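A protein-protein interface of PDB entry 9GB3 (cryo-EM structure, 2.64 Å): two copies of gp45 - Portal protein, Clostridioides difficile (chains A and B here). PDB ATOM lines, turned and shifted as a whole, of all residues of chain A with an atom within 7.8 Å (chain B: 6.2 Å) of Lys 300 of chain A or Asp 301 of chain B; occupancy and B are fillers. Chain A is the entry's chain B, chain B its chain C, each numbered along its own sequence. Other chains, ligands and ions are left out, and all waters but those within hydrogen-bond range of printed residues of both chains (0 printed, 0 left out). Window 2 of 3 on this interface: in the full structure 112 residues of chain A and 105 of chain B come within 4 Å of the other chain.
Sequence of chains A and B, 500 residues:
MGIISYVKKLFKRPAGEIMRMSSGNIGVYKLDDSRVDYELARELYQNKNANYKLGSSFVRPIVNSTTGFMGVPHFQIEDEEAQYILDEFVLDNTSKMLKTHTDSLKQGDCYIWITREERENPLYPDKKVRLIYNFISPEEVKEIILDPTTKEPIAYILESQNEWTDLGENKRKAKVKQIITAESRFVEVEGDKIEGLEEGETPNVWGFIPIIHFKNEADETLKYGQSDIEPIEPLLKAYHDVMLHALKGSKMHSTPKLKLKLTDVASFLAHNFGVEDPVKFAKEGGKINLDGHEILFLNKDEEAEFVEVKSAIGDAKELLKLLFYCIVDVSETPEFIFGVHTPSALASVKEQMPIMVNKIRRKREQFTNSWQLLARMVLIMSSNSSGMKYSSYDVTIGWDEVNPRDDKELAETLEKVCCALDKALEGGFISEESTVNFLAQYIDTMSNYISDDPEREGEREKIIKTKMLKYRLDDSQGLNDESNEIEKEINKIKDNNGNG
O of Leu 298 of chain A is in hydrogen-bond range of N of Leu 262 of chain B, at 2.7 Å. The side-chain amino group (NZ) of Lys 261 of chain B lies within salt-bridge range of the side-chain carboxylate (OE1) of Glu 303 of chain A. NZ of Lys 300 of chain A is in salt-bridge range of OD2 of Asp 301 of chain B (3.7 Å).
OD1 of Asn 299 of chain A lies close to OE2 of Glu 302 of chain A (2.8 Å). The side-chain carboxylate (OE2) of Glu 302 of chain A lies within hydrogen-bond range of the backbone NH (N) of Thr 263 of chain A. N of Lys 261 of chain B lies within hydrogen-bond range of O of Glu 303 of chain B (2.7 Å). The side-chain carboxylate (OE2) of Glu 302 of chain B is in hydrogen-bond range of the backbone NH (N) of Thr 263 of chain B (3.2 Å).
Among the printed residues, pairs that only touch across the chains: Leu 298 of chain A with Lys 261 of chain B (3.4 Å), Asn 299 of chain A with Lys 261 of chain B (3.4 Å), Asn 299 of chain A with Leu 262 of chain B (3.5 Å), Lys 300 of chain A with Lys 261 of chain B (3.1 Å), Lys 300 of chain A with Leu 262 of chain B (3.6 Å), Lys 300 of chain A with Thr 263 of chain B (3.1 Å) and Glu 302 of chain A with Lys 261 of chain B (3.3 Å).
Thr 263 of chain A touches none of the printed residues of chain B. Of the printed residues of chain B, Leu 298 of chain A touches Lys 261 (3.4 Å) and Leu 262 (2.7 Å). Printed residues of chain B within 4 Å of Asn 299 of chain A: Lys 261 (3.4 Å) and Leu 262 (3.5 Å). Of the printed residues of chain B, Lys 300 of chain A touches Lys 261, Leu 262, Thr 263 and Asp 301. Of the printed residues of chain B, Glu 302 of chain A touches Lys 261 (3.3 Å). Printed residues of chain B within 4 Å of Glu 303 of chain A: Lys 261 (3.3 Å). Of the printed residues of chain A, Thr 263 of chain B touches Lys 300 (3.1 Å). Lys 300 of chain B touches none of the printed residues of chain A. Of chain A, only Lys 300 comes within 4 Å of Asp 301 of chain B. The nearest residue of chain B that does not touch Lys 300 of chain A is Glu 302 of chain B (5.1 Å).
Printed residues of chain B that touch a printed residue of chain A: Lys 261, Leu 262, Thr 263 and Asp 301. Hydrophobic or aromatic side chains of chain B within 4 Å of the printed part of chain A: Leu 262. Along chain B the printed residues that touch a printed residue of chain A span positions 261 to 301. Printed residues of chain A that touch a printed residue of chain B: Leu 298, Asn 299, Lys 300, Glu 302 and Glu 303. Among the printed residues, 10 pairs touch across the chains. Among the printed residues, Asp or Glu carboxylates within 4 Å of a Lys or Arg side-chain nitrogen of the other chain: Lys 300 of chain A with Asp 301 of chain B and Glu 303 of chain A with Lys 261 of chain B.
Lys 300 of chain A touches Thr 263 of chain B, but with the chains exchanged Thr 263 of chain A does not touch Lys 300 of chain B (17.3 Å). Lys 300 of chain A touches Asp 301 of chain B, but with the chains exchanged Asp 301 of chain A does not touch Lys 300 of chain B (11.6 Å). Of the 10 pairs that touch across the chains among the printed residues, none has its exchanged pair printed and touching as well.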
ATOM      1  N   THR A 263      -2.654 -39.844  -6.727  1.00  0.00           N
ATOM      2  CA  THR A 263      -3.990 -40.332  -6.406  1.00  0.00           C
ATOM      3  C   THR A 263      -4.272 -41.656  -7.107  1.00  0.00           C
ATOM      4  O   THR A 263      -4.860 -42.566  -6.514  1.00  0.00           O
ATOM      5  CB  THR A 263      -5.037 -39.286  -6.786  1.00  0.00           C
ATOM      6  OG1 THR A 263      -4.882 -38.130  -5.953  1.00  0.00           O
ATOM      7  CG2 THR A 263      -6.444 -39.837  -6.612  1.00  0.00           C
ATOM      8  N   LEU A 298       0.317 -31.310 -10.334  1.00  0.00           N
ATOM      9  CA  LEU A 298      -0.289 -32.311  -9.472  1.00  0.00           C
ATOM     10  C   LEU A 298      -1.488 -31.714  -8.749  1.00  0.00           C
ATOM     11  O   LEU A 298      -1.743 -30.509  -8.803  1.00  0.00           O
ATOM     12  CB  LEU A 298       0.728 -32.844  -8.455  1.00  0.00           C
ATOM     13  CG  LEU A 298       2.069 -33.331  -9.005  1.00  0.00           C
ATOM     14  CD1 LEU A 298       2.997 -33.694  -7.864  1.00  0.00           C
ATOM     15  CD2 LEU A 298       1.878 -34.518  -9.932  1.00  0.00           C
ATOM     16  N   ASN A 299      -2.228 -32.580  -8.067  1.00  0.00           N
ATOM     17  CA  ASN A 299      -3.368 -32.163  -7.269  1.00  0.00           C
ATOM     18  C   ASN A 299      -2.911 -31.767  -5.869  1.00  0.00           C
ATOM     19  O   ASN A 299      -1.730 -31.836  -5.528  1.00  0.00           O
ATOM     20  CB  ASN A 299      -4.410 -33.279  -7.195  1.00  0.00           C
ATOM     21  CG  ASN A 299      -4.625 -33.964  -8.528  1.00  0.00           C
ATOM     22  OD1 ASN A 299      -4.446 -35.174  -8.652  1.00  0.00           O
ATOM     23  ND2 ASN A 299      -5.012 -33.190  -9.534  1.00  0.00           N
ATOM     24  N   LYS A 300      -3.875 -31.339  -5.051  1.00  0.00           N
ATOM     25  CA  LYS A 300      -3.555 -30.899  -3.697  1.00  0.00           C
ATOM     26  C   LYS A 300      -2.981 -32.037  -2.864  1.00  0.00           C
ATOM     27  O   LYS A 300      -2.024 -31.839  -2.108  1.00  0.00           O
ATOM     28  CB  LYS A 300      -4.805 -30.339  -3.021  1.00  0.00           C
ATOM     29  CG  LYS A 300      -5.163 -28.922  -3.418  1.00  0.00           C
ATOM     30  CD  LYS A 300      -6.326 -28.416  -2.563  1.00  0.00           C
ATOM     31  CE  LYS A 300      -7.246 -27.438  -3.291  1.00  0.00           C
ATOM     32  NZ  LYS A 300      -8.648 -27.534  -2.800  1.00  0.00           N
ATOM     33  N   ASP A 301      -3.559 -33.232  -2.981  1.00  0.00           N
ATOM     34  CA  ASP A 301      -3.186 -34.341  -2.113  1.00  0.00           C
ATOM     35  C   ASP A 301      -1.921 -35.060  -2.564  1.00  0.00           C
ATOM     36  O   ASP A 301      -1.301 -35.751  -1.750  1.00  0.00           O
ATOM     37  CB  ASP A 301      -4.336 -35.346  -2.034  1.00  0.00           C
ATOM     38  CG  ASP A 301      -5.558 -34.785  -1.333  1.00  0.00           C
ATOM     39  OD1 ASP A 301      -5.431 -33.756  -0.635  1.00  0.00           O
ATOM     40  OD2 ASP A 301      -6.647 -35.378  -1.476  1.00  0.00           O
ATOM     41  N   GLU A 302      -1.526 -34.919  -3.825  1.00  0.00           N
ATOM     42  CA  GLU A 302      -0.374 -35.642  -4.338  1.00  0.00           C
ATOM     43  C   GLU A 302       0.925 -34.962  -3.911  1.00  0.00           C
ATOM     44  O   GLU A 302       0.944 -33.822  -3.444  1.00  0.00           O
ATOM     45  CB  GLU A 302      -0.451 -35.748  -5.858  1.00  0.00           C
ATOM     46  CG  GLU A 302      -1.789 -36.246  -6.370  1.00  0.00           C
ATOM     47  CD  GLU A 302      -1.751 -36.625  -7.834  1.00  0.00           C
ATOM     48  OE1 GLU A 302      -0.797 -36.222  -8.529  1.00  0.00           O
ATOM     49  OE2 GLU A 302      -2.677 -37.327  -8.293  1.00  0.00           O
ATOM     50  N   GLU A 303       2.028 -35.688  -4.083  1.00  0.00           N
ATOM     51  CA  GLU A 303       3.336 -35.239  -3.636  1.00  0.00           C
ATOM     52  C   GLU A 303       4.392 -35.796  -4.576  1.00  0.00           C
ATOM     53  O   GLU A 303       4.274 -36.929  -5.047  1.00  0.00           O
ATOM     54  CB  GLU A 303       3.604 -35.693  -2.194  1.00  0.00           C
ATOM     55  CG  GLU A 303       4.898 -35.179  -1.570  1.00  0.00           C
ATOM     56  CD  GLU A 303       4.873 -33.690  -1.303  1.00  0.00           C
ATOM     57  OE1 GLU A 303       3.834 -33.182  -0.834  1.00  0.00           O
ATOM     58  OE2 GLU A 303       5.897 -33.026  -1.559  1.00  0.00           O
ATOM     59  N   LYS B 261       1.001 -27.911  -7.026  1.00  0.00           N
ATOM     60  CA  LYS B 261      -0.115 -28.673  -6.473  1.00  0.00           C
ATOM     61  C   LYS B 261      -1.355 -27.800  -6.610  1.00  0.00           C
ATOM     62  O   LYS B 261      -1.586 -26.898  -5.802  1.00  0.00           O
ATOM     63  CB  LYS B 261       0.160 -29.063  -5.025  1.00  0.00           C
ATOM     64  CG  LYS B 261       1.146 -30.214  -4.890  1.00  0.00           C
ATOM     65  CD  LYS B 261       1.810 -30.248  -3.524  1.00  0.00           C
ATOM     66  CE  LYS B 261       0.836 -30.637  -2.431  1.00  0.00           C
ATOM     67  NZ  LYS B 261       1.525 -30.835  -1.128  1.00  0.00           N
ATOM     68  N   LEU B 262      -2.151 -28.077  -7.638  1.00  0.00           N
ATOM     69  CA  LEU B 262      -3.227 -27.201  -8.076  1.00  0.00           C
ATOM     70  C   LEU B 262      -4.581 -27.797  -7.719  1.00  0.00           C
ATOM     71  O   LEU B 262      -4.744 -29.017  -7.644  1.00  0.00           O
ATOM     72  CB  LEU B 262      -3.151 -26.968  -9.586  1.00  0.00           C
ATOM     73  CG  LEU B 262      -1.851 -26.351 -10.106  1.00  0.00           C
ATOM     74  CD1 LEU B 262      -1.685 -26.641 -11.583  1.00  0.00           C
ATOM     75  CD2 LEU B 262      -1.830 -24.858  -9.842  1.00  0.00           C
ATOM     76  N   THR B 263      -5.556 -26.914  -7.496  1.00  0.00           N
ATOM     77  CA  THR B 263      -6.913 -27.368  -7.215  1.00  0.00           C
ATOM     78  C   THR B 263      -7.507 -28.096  -8.414  1.00  0.00           C
ATOM     79  O   THR B 263      -8.178 -29.122  -8.258  1.00  0.00           O
ATOM     80  CB  THR B 263      -7.792 -26.181  -6.821  1.00  0.00           C
ATOM     81  OG1 THR B 263      -7.222 -25.516  -5.688  1.00  0.00           O
ATOM     82  CG2 THR B 263      -9.198 -26.644  -6.473  1.00  0.00           C
ATOM     83  N   ASN B 299      -4.252 -19.901  -5.240  1.00  0.00           N
ATOM     84  CA  ASN B 299      -5.242 -19.801  -4.182  1.00  0.00           C
ATOM     85  C   ASN B 299      -4.606 -20.134  -2.836  1.00  0.00           C
ATOM     86  O   ASN B 299      -3.426 -20.476  -2.742  1.00  0.00           O
ATOM     87  CB  ASN B 299      -6.420 -20.731  -4.460  1.00  0.00           C
ATOM     88  CG  ASN B 299      -6.858 -20.699  -5.907  1.00  0.00           C
ATOM     89  OD1 ASN B 299      -6.859 -21.723  -6.590  1.00  0.00           O
ATOM     90  ND2 ASN B 299      -7.230 -19.520  -6.386  1.00  0.00           N
ATOM     91  N   LYS B 300      -5.412 -20.026  -1.778  1.00  0.00           N
ATOM     92  CA  LYS B 300      -4.914 -20.314  -0.438  1.00  0.00           C
ATOM     93  C   LYS B 300      -4.476 -21.766  -0.312  1.00  0.00           C
ATOM     94  O   LYS B 300      -3.448 -22.061   0.307  1.00  0.00           O
ATOM     95  CB  LYS B 300      -5.990 -20.006   0.601  1.00  0.00           C
ATOM     96  CG  LYS B 300      -6.354 -18.540   0.733  1.00  0.00           C
ATOM     97  CD  LYS B 300      -7.451 -18.362   1.771  1.00  0.00           C
ATOM     98  CE  LYS B 300      -7.897 -16.917   1.886  1.00  0.00           C
ATOM     99  NZ  LYS B 300      -9.009 -16.754   2.863  1.00  0.00           N
ATOM    100  N   ASP B 301      -5.248 -22.688  -0.887  1.00  0.00           N
ATOM    101  CA  ASP B 301      -4.997 -24.111  -0.707  1.00  0.00           C
ATOM    102  C   ASP B 301      -3.931 -24.660  -1.646  1.00  0.00           C
ATOM    103  O   ASP B 301      -3.428 -25.762  -1.406  1.00  0.00           O
ATOM    104  CB  ASP B 301      -6.297 -24.890  -0.910  1.00  0.00           C
ATOM    105  CG  ASP B 301      -7.315 -24.627   0.182  1.00  0.00           C
ATOM    106  OD1 ASP B 301      -6.979 -23.931   1.163  1.00  0.00           O
ATOM    107  OD2 ASP B 301      -8.456 -25.120   0.058  1.00  0.00           O
ATOM    108  N   GLU B 302      -3.574 -23.930  -2.698  1.00  0.00           N
ATOM    109  CA  GLU B 302      -2.616 -24.427  -3.672  1.00  0.00           C
ATOM    110  C   GLU B 302      -1.187 -24.199  -3.187  1.00  0.00           C
ATOM    111  O   GLU B 302      -0.930 -23.443  -2.248  1.00  0.00           O
ATOM    112  CB  GLU B 302      -2.841 -23.757  -5.023  1.00  0.00           C
ATOM    113  CG  GLU B 302      -4.128 -24.183  -5.701  1.00  0.00           C
ATOM    114  CD  GLU B 302      -4.376 -23.446  -6.998  1.00  0.00           C
ATOM    115  OE1 GLU B 302      -3.562 -22.569  -7.349  1.00  0.00           O
ATOM    116  OE2 GLU B 302      -5.384 -23.747  -7.671  1.00  0.00           O
ATOM    117  N   GLU B 303      -0.247 -24.872  -3.846  1.00  0.00           N
ATOM    118  CA  GLU B 303       1.148 -24.862  -3.431  1.00  0.00           C
ATOM    119  C   GLU B 303       2.032 -24.996  -4.661  1.00  0.00           C
ATOM    120  O   GLU B 303       1.687 -25.711  -5.605  1.00  0.00           O
ATOM    121  CB  GLU B 303       1.422 -26.001  -2.437  1.00  0.00           C
ATOM    122  CG  GLU B 303       2.834 -26.058  -1.873  1.00  0.00           C
ATOM    123  CD  GLU B 303       3.180 -24.847  -1.034  1.00  0.00           C
ATOM    124  OE1 GLU B 303       2.439 -24.552  -0.074  1.00  0.00           O
ATOM    125  OE2 GLU B 303       4.199 -24.193  -1.334  1.00  0.00           O
